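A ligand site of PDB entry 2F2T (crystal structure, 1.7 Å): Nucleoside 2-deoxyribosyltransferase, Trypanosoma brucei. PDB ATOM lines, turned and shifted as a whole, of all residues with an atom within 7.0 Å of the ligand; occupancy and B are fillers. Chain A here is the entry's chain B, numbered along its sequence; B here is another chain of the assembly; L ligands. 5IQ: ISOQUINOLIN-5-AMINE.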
ATOM      1  N   ARG A 125      28.489   6.149  -6.987  1.00  0.00           N
ATOM      2  CA  ARG A 125      28.364   7.490  -7.538  1.00  0.00           C
ATOM      3  C   ARG A 125      28.461   8.586  -6.479  1.00  0.00           C
ATOM      4  O   ARG A 125      27.859   8.482  -5.404  1.00  0.00           O
ATOM      5  CB  ARG A 125      27.067   7.627  -8.329  1.00  0.00           C
ATOM      6  CG  ARG A 125      26.997   6.740  -9.577  1.00  0.00           C
ATOM      7  CD  ARG A 125      25.645   6.875 -10.292  1.00  0.00           C
ATOM      8  NE  ARG A 125      25.271   8.273 -10.525  1.00  0.00           N
ATOM      9  CZ  ARG A 125      25.679   9.005 -11.556  1.00  0.00           C
ATOM     10  NH1 ARG A 125      26.497   8.498 -12.483  1.00  0.00           N
ATOM     11  NH2 ARG A 125      25.275  10.262 -11.667  1.00  0.00           N
ATOM     12  N   GLU A 127      27.633  12.539  -5.931  1.00  0.00           N
ATOM     13  CA  GLU A 127      26.721  13.554  -6.470  1.00  0.00           C
ATOM     14  C   GLU A 127      27.462  14.695  -7.175  1.00  0.00           C
ATOM     15  O   GLU A 127      28.533  15.110  -6.736  1.00  0.00           O
ATOM     16  CB  GLU A 127      25.824  14.130  -5.373  1.00  0.00           C
ATOM     17  CG  GLU A 127      24.807  13.142  -4.826  1.00  0.00           C
ATOM     18  CD  GLU A 127      23.910  13.723  -3.751  1.00  0.00           C
ATOM     19  OE1 GLU A 127      23.712  14.956  -3.725  1.00  0.00           O
ATOM     20  OE2 GLU A 127      23.408  12.939  -2.928  1.00  0.00           O
ATOM     21  N   GLY A 128      26.875  15.176  -8.269  1.00  0.00           N
ATOM     22  CA  GLY A 128      27.473  16.241  -9.072  1.00  0.00           C
ATOM     23  C   GLY A 128      26.563  17.442  -9.211  1.00  0.00           C
ATOM     24  O   GLY A 128      26.165  17.805 -10.322  1.00  0.00           O
ATOM     25  N   PHE A 129      26.233  18.055  -8.073  1.00  0.00           N
ATOM     26  CA  PHE A 129      25.347  19.209  -8.050  1.00  0.00           C
ATOM     27  C   PHE A 129      26.035  20.455  -7.497  1.00  0.00           C
ATOM     28  O   PHE A 129      25.373  21.428  -7.139  1.00  0.00           O
ATOM     29  CB  PHE A 129      24.073  18.890  -7.257  1.00  0.00           C
ATOM     30  CG  PHE A 129      23.199  17.860  -7.910  1.00  0.00           C
ATOM     31  CD1 PHE A 129      22.190  18.250  -8.792  1.00  0.00           C
ATOM     32  CD2 PHE A 129      23.384  16.503  -7.664  1.00  0.00           C
ATOM     33  CE1 PHE A 129      21.379  17.309  -9.406  1.00  0.00           C
ATOM     34  CE2 PHE A 129      22.579  15.548  -8.276  1.00  0.00           C
ATOM     35  CZ  PHE A 129      21.576  15.950  -9.152  1.00  0.00           C
ATOM     36  N   ASN A 134      25.238  15.491   0.560  1.00  0.00           N
ATOM     37  CA  ASN A 134      23.983  14.986   0.005  1.00  0.00           C
ATOM     38  C   ASN A 134      22.977  16.118  -0.223  1.00  0.00           C
ATOM     39  O   ASN A 134      22.708  16.904   0.684  1.00  0.00           O
ATOM     40  CB  ASN A 134      23.403  13.921   0.940  1.00  0.00           C
ATOM     41  CG  ASN A 134      22.250  13.158   0.313  1.00  0.00           C
ATOM     42  OD1 ASN A 134      21.192  13.723   0.054  1.00  0.00           O
ATOM     43  ND2 ASN A 134      22.460  11.866   0.077  1.00  0.00           N
ATOM     44  N   LEU A 135      22.432  16.183  -1.434  1.00  0.00           N
ATOM     45  CA  LEU A 135      21.560  17.301  -1.837  1.00  0.00           C
ATOM     46  C   LEU A 135      20.312  17.495  -0.963  1.00  0.00           C
ATOM     47  O   LEU A 135      19.771  18.600  -0.903  1.00  0.00           O
ATOM     48  CB  LEU A 135      21.178  17.197  -3.331  1.00  0.00           C
ATOM     49  CG  LEU A 135      20.306  16.038  -3.820  1.00  0.00           C
ATOM     50  CD1 LEU A 135      18.828  16.335  -3.651  1.00  0.00           C
ATOM     51  CD2 LEU A 135      20.621  15.734  -5.274  1.00  0.00           C
ATOM     52  N   MET A 136      19.856  16.426  -0.297  1.00  0.00           N
ATOM     53  CA  MET A 136      18.705  16.527   0.607  1.00  0.00           C
ATOM     54  C   MET A 136      18.966  17.520   1.745  1.00  0.00           C
ATOM     55  O   MET A 136      18.031  18.109   2.292  1.00  0.00           O
ATOM     56  CB  MET A 136      18.340  15.152   1.183  1.00  0.00           C
ATOM     57  CG  MET A 136      17.890  14.116   0.150  1.00  0.00           C
ATOM     58  SD  MET A 136      16.431  14.723  -1.002  1.00  0.00           S
ATOM     59  CE  MET A 136      15.036  14.911   0.327  1.00  0.00           C
ATOM     60  N   TYR B  13       7.455   5.182   0.048  1.00  0.00           N
ATOM     61  CA  TYR B  13       8.657   5.905  -0.346  1.00  0.00           C
ATOM     62  C   TYR B  13       9.874   5.012  -0.167  1.00  0.00           C
ATOM     63  O   TYR B  13      10.110   4.479   0.914  1.00  0.00           O
ATOM     64  CB  TYR B  13       8.812   7.208   0.444  1.00  0.00           C
ATOM     65  CG  TYR B  13      10.046   8.002   0.069  1.00  0.00           C
ATOM     66  CD1 TYR B  13      10.114   8.666  -1.163  1.00  0.00           C
ATOM     67  CD2 TYR B  13      11.129   8.089   0.934  1.00  0.00           C
ATOM     68  CE1 TYR B  13      11.248   9.394  -1.511  1.00  0.00           C
ATOM     69  CE2 TYR B  13      12.266   8.827   0.584  1.00  0.00           C
ATOM     70  CZ  TYR B  13      12.315   9.467  -0.639  1.00  0.00           C
ATOM     71  OH  TYR B  13      13.427  10.194  -0.982  1.00  0.00           O
ATOM     72  N   VAL B  19      20.444   4.548  -5.162  1.00  0.00           N
ATOM     73  CA  VAL B  19      20.609   5.586  -6.174  1.00  0.00           C
ATOM     74  C   VAL B  19      22.078   5.821  -6.574  1.00  0.00           C
ATOM     75  O   VAL B  19      22.361   6.276  -7.684  1.00  0.00           O
ATOM     76  CB  VAL B  19      19.935   6.925  -5.726  1.00  0.00           C
ATOM     77  CG1 VAL B  19      20.576   7.466  -4.450  1.00  0.00           C
ATOM     78  CG2 VAL B  19      19.983   7.975  -6.839  1.00  0.00           C
ATOM     79  N   PHE B  20      22.992   5.483  -5.671  1.00  0.00           N
ATOM     80  CA  PHE B  20      24.427   5.683  -5.898  1.00  0.00           C
ATOM     81  C   PHE B  20      25.126   4.469  -6.526  1.00  0.00           C
ATOM     82  O   PHE B  20      26.322   4.535  -6.826  1.00  0.00           O
ATOM     83  CB  PHE B  20      25.126   6.127  -4.614  1.00  0.00           C
ATOM     84  CG  PHE B  20      24.488   7.325  -3.965  1.00  0.00           C
ATOM     85  CD1 PHE B  20      24.416   8.544  -4.637  1.00  0.00           C
ATOM     86  CD2 PHE B  20      23.959   7.247  -2.682  1.00  0.00           C
ATOM     87  CE1 PHE B  20      23.819   9.652  -4.051  1.00  0.00           C
ATOM     88  CE2 PHE B  20      23.352   8.351  -2.083  1.00  0.00           C
ATOM     89  CZ  PHE B  20      23.287   9.564  -2.765  1.00  0.00           C
ATOM     90  N   MET B  24      22.512   3.584 -11.093  1.00  0.00           N
ATOM     91  CA  MET B  24      21.620   4.575 -10.486  1.00  0.00           C
ATOM     92  C   MET B  24      20.444   3.952  -9.732  1.00  0.00           C
ATOM     93  O   MET B  24      19.418   4.594  -9.522  1.00  0.00           O
ATOM     94  CB  MET B  24      21.128   5.590 -11.531  1.00  0.00           C
ATOM     95  CG  MET B  24      22.227   6.435 -12.159  1.00  0.00           C
ATOM     96  SD  MET B  24      21.525   7.709 -13.443  1.00  0.00           S
ATOM     97  CE  MET B  24      20.482   8.842 -12.225  1.00  0.00           C
ATOM     98  N   TYR B  29      15.629  -0.898  -7.682  1.00  0.00           N
ATOM     99  CA  TYR B  29      14.301  -0.337  -7.920  1.00  0.00           C
ATOM    100  C   TYR B  29      13.410  -1.275  -8.726  1.00  0.00           C
ATOM    101  O   TYR B  29      12.218  -1.375  -8.461  1.00  0.00           O
ATOM    102  CB  TYR B  29      14.382   1.040  -8.578  1.00  0.00           C
ATOM    103  CG  TYR B  29      15.029   2.107  -7.713  1.00  0.00           C
ATOM    104  CD1 TYR B  29      14.750   2.208  -6.338  1.00  0.00           C
ATOM    105  CD2 TYR B  29      15.904   3.045  -8.268  1.00  0.00           C
ATOM    106  CE1 TYR B  29      15.343   3.202  -5.560  1.00  0.00           C
ATOM    107  CE2 TYR B  29      16.495   4.037  -7.500  1.00  0.00           C
ATOM    108  CZ  TYR B  29      16.211   4.103  -6.137  1.00  0.00           C
ATOM    109  OH  TYR B  29      16.800   5.093  -5.378  1.00  0.00           O
ATOM    110  N   PRO B  46      12.992   7.809  -5.509  1.00  0.00           N
ATOM    111  CA  PRO B  46      13.713   9.090  -5.527  1.00  0.00           C
ATOM    112  C   PRO B  46      14.114   9.607  -6.909  1.00  0.00           C
ATOM    113  O   PRO B  46      14.172  10.822  -7.106  1.00  0.00           O
ATOM    114  CB  PRO B  46      14.960   8.794  -4.699  1.00  0.00           C
ATOM    115  CG  PRO B  46      14.491   7.770  -3.715  1.00  0.00           C
ATOM    116  CD  PRO B  46      13.571   6.890  -4.516  1.00  0.00           C
ATOM    117  N   THR B  47      14.363   8.704  -7.859  1.00  0.00           N
ATOM    118  CA  THR B  47      14.826   9.091  -9.194  1.00  0.00           C
ATOM    119  C   THR B  47      13.708   9.242 -10.230  1.00  0.00           C
ATOM    120  O   THR B  47      13.982   9.586 -11.387  1.00  0.00           O
ATOM    121  CB  THR B  47      15.864   8.088  -9.737  1.00  0.00           C
ATOM    122  OG1 THR B  47      15.314   6.762  -9.696  1.00  0.00           O
ATOM    123  CG2 THR B  47      17.152   8.136  -8.931  1.00  0.00           C
ATOM    124  N   GLU B  50      13.047  12.582 -12.619  1.00  0.00           N
ATOM    125  CA  GLU B  50      14.059  13.381 -11.936  1.00  0.00           C
ATOM    126  C   GLU B  50      14.312  14.732 -12.617  1.00  0.00           C
ATOM    127  O   GLU B  50      14.518  14.795 -13.833  1.00  0.00           O
ATOM    128  CB  GLU B  50      15.379  12.611 -11.776  1.00  0.00           C
ATOM    129  CG  GLU B  50      16.388  13.296 -10.858  1.00  0.00           C
ATOM    130  CD  GLU B  50      17.590  12.427 -10.544  1.00  0.00           C
ATOM    131  OE1 GLU B  50      17.403  11.328  -9.976  1.00  0.00           O
ATOM    132  OE2 GLU B  50      18.726  12.851 -10.836  1.00  0.00           O
ATOM    133  N   ILE B  57      14.806  18.383  -7.102  1.00  0.00           N
ATOM    134  CA  ILE B  57      14.904  16.961  -6.738  1.00  0.00           C
ATOM    135  C   ILE B  57      14.551  16.767  -5.260  1.00  0.00           C
ATOM    136  O   ILE B  57      13.767  15.885  -4.917  1.00  0.00           O
ATOM    137  CB  ILE B  57      16.322  16.396  -7.023  1.00  0.00           C
ATOM    138  CG1 ILE B  57      16.625  16.448  -8.521  1.00  0.00           C
ATOM    139  CG2 ILE B  57      16.451  14.968  -6.497  1.00  0.00           C
ATOM    140  CD1 ILE B  57      18.051  16.089  -8.886  1.00  0.00           C
ATOM    141  N   ARG B  58      15.118  17.617  -4.402  1.00  0.00           N
ATOM    142  CA  ARG B  58      14.828  17.570  -2.982  1.00  0.00           C
ATOM    143  C   ARG B  58      13.336  17.796  -2.699  1.00  0.00           C
ATOM    144  O   ARG B  58      12.725  17.033  -1.939  1.00  0.00           O
ATOM    145  CB  ARG B  58      15.673  18.605  -2.239  1.00  0.00           C
ATOM    146  CG  ARG B  58      15.431  18.674  -0.740  1.00  0.00           C
ATOM    147  CD  ARG B  58      16.334  19.700  -0.103  1.00  0.00           C
ATOM    148  NE  ARG B  58      16.027  19.903   1.319  1.00  0.00           N
ATOM    149  CZ  ARG B  58      15.096  20.749   1.766  1.00  0.00           C
ATOM    150  NH1 ARG B  58      14.373  21.478   0.922  1.00  0.00           N
ATOM    151  NH2 ARG B  58      14.893  20.869   3.078  1.00  0.00           N
ATOM    152  N   ASN B  61      11.192  14.832  -3.630  1.00  0.00           N
ATOM    153  CA  ASN B  61      11.380  13.745  -2.679  1.00  0.00           C
ATOM    154  C   ASN B  61      10.684  13.987  -1.344  1.00  0.00           C
ATOM    155  O   ASN B  61      10.092  13.071  -0.775  1.00  0.00           O
ATOM    156  CB  ASN B  61      12.862  13.437  -2.479  1.00  0.00           C
ATOM    157  CG  ASN B  61      13.405  12.488  -3.518  1.00  0.00           C
ATOM    158  OD1 ASN B  61      13.514  11.290  -3.279  1.00  0.00           O
ATOM    159  ND2 ASN B  61      13.726  13.006  -4.703  1.00  0.00           N
ATOM    160  N   ASP B  84      23.472   5.977   5.067  1.00  0.00           N
ATOM    161  CA  ASP B  84      23.473   7.133   4.172  1.00  0.00           C
ATOM    162  C   ASP B  84      22.741   8.324   4.792  1.00  0.00           C
ATOM    163  O   ASP B  84      21.613   8.176   5.272  1.00  0.00           O
ATOM    164  CB  ASP B  84      22.832   6.742   2.842  1.00  0.00           C
ATOM    165  CG  ASP B  84      22.476   7.942   1.987  1.00  0.00           C
ATOM    166  OD1 ASP B  84      23.350   8.799   1.744  1.00  0.00           O
ATOM    167  OD2 ASP B  84      21.315   8.001   1.538  1.00  0.00           O
ATOM    168  N   GLY B  86      21.444  10.965   3.343  1.00  0.00           N
ATOM    169  CA  GLY B  86      20.269  11.345   2.553  1.00  0.00           C
ATOM    170  C   GLY B  86      19.060  10.538   2.988  1.00  0.00           C
ATOM    171  O   GLY B  86      17.970  11.084   3.172  1.00  0.00           O
ATOM    172  N   THR B  87      19.280   9.235   3.162  1.00  0.00           N
ATOM    173  CA  THR B  87      18.273   8.328   3.698  1.00  0.00           C
ATOM    174  C   THR B  87      17.885   8.730   5.126  1.00  0.00           C
ATOM    175  O   THR B  87      16.712   8.727   5.481  1.00  0.00           O
ATOM    176  CB  THR B  87      18.770   6.871   3.664  1.00  0.00           C
ATOM    177  OG1 THR B  87      19.208   6.558   2.331  1.00  0.00           O
ATOM    178  CG2 THR B  87      17.666   5.904   4.068  1.00  0.00           C
ATOM    179  N   GLU B  90      15.594  11.620   5.111  1.00  0.00           N
ATOM    180  CA  GLU B  90      14.246  11.185   4.709  1.00  0.00           C
ATOM    181  C   GLU B  90      13.483  10.487   5.825  1.00  0.00           C
ATOM    182  O   GLU B  90      12.268  10.666   5.961  1.00  0.00           O
ATOM    183  CB  GLU B  90      14.352  10.300   3.463  1.00  0.00           C
ATOM    184  CG  GLU B  90      14.695  11.110   2.208  1.00  0.00           C
ATOM    185  CD  GLU B  90      15.633  10.397   1.258  1.00  0.00           C
ATOM    186  OE1 GLU B  90      15.783   9.164   1.358  1.00  0.00           O
ATOM    187  OE2 GLU B  90      16.226  11.095   0.411  1.00  0.00           O
HETATM  188  CAB 5IQ L   1      19.872  12.015  -4.923  1.00  0.00           C
HETATM  189  CAF 5IQ L   1      21.184  11.992  -5.377  1.00  0.00           C
HETATM  190  CAK 5IQ L   1      21.444  11.699  -6.715  1.00  0.00           C
HETATM  191  NAH 5IQ L   1      20.439  11.448  -7.552  1.00  0.00           N
HETATM  192  CAD 5IQ L   1      19.169  11.460  -7.157  1.00  0.00           C
HETATM  193  CAA 5IQ L   1      18.850  11.748  -5.836  1.00  0.00           C
HETATM  194  CAC 5IQ L   1      17.518  11.764  -5.428  1.00  0.00           C
HETATM  195  CAG 5IQ L   1      17.202  12.054  -4.097  1.00  0.00           C
HETATM  196  CAI 5IQ L   1      18.227  12.331  -3.187  1.00  0.00           C
HETATM  197  CAE 5IQ L   1      19.559  12.314  -3.594  1.00  0.00           C
HETATM  198  NAJ 5IQ L   1      20.520  12.574  -2.708  1.00  0.00           N
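The side-chain carboxylate (OE2) of Glu 127 sits at hydrogen-bond distance from a nitrogen (NAJ) of the ligand, at 2.9 Å.
NAJ of the ligand sits at hydrogen-bond distance from OD1 of Asn 134.
OE2 of Glu 127 is in hydrogen-bond range of ND2 of Asn 134.
The side-chain carboxylate of Glu 127 sits at hydrogen-bond distance from the backbone NH of Leu 135 (2.9 Å).
OD1 of Asn 134 lies within hydrogen-bond range of N of Met 136 (3.0 Å).
The side-chain amide nitrogen (ND2) of Asn 61 of chain B sits at hydrogen-bond distance from the backbone carbonyl oxygen (O) of Ile 57 of chain B (2.9 Å).
The side-chain amide nitrogen (ND2) of Asn 61 of chain B lies within hydrogen-bond range of the backbone carbonyl oxygen (O) of Pro 46 of chain B, at 3.3 Å.
The side-chain amide oxygen (OD1) of Asn 61 of chain B is in hydrogen-bond range of the side-chain hydroxyl (OH) of Tyr 13 of chain B, at 2.5 Å.
The backbone carbonyl oxygen of Met 136 is in hydrogen-bond range of the guanidinium group of Arg 58 of chain B, 2.9 Å away.
N of Arg 125 sits at hydrogen-bond distance from O of Phe 20 of chain B, 2.7 Å away.
Leu 135 touches the ligand.
Met 136 touches the ligand (SD to CAI, 3.7 Å).
Val 19 of chain B touches the ligand.
Phe 20 of chain B touches the ligand.
O of Pro 46 of chain B touches CAC of the ligand, at 3.9 Å.
Glu 50 of chain B touches the ligand (OE1 to CAD, 3.3 Å).
Ile 57 of chain B touches the ligand (CG2 to CAC, 3.5 Å).
Asn 61 of chain B touches the ligand.
Hydrophobic or aromatic side chains within 4 Å of the ligand: Leu 135, Met 136, Val 19 of chain B, Phe 20 of chain B, Pro 46 of chain B and Ile 57 of chain B.
Within 4 Å of the ligand: Glu 127, Asn 134, Leu 135, Met 136, Val 19 of chain B, Phe 20 of chain B, Pro 46 of chain B, Glu 50 of chain B, Ile 57 of chain B and Asn 61 of chain B.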
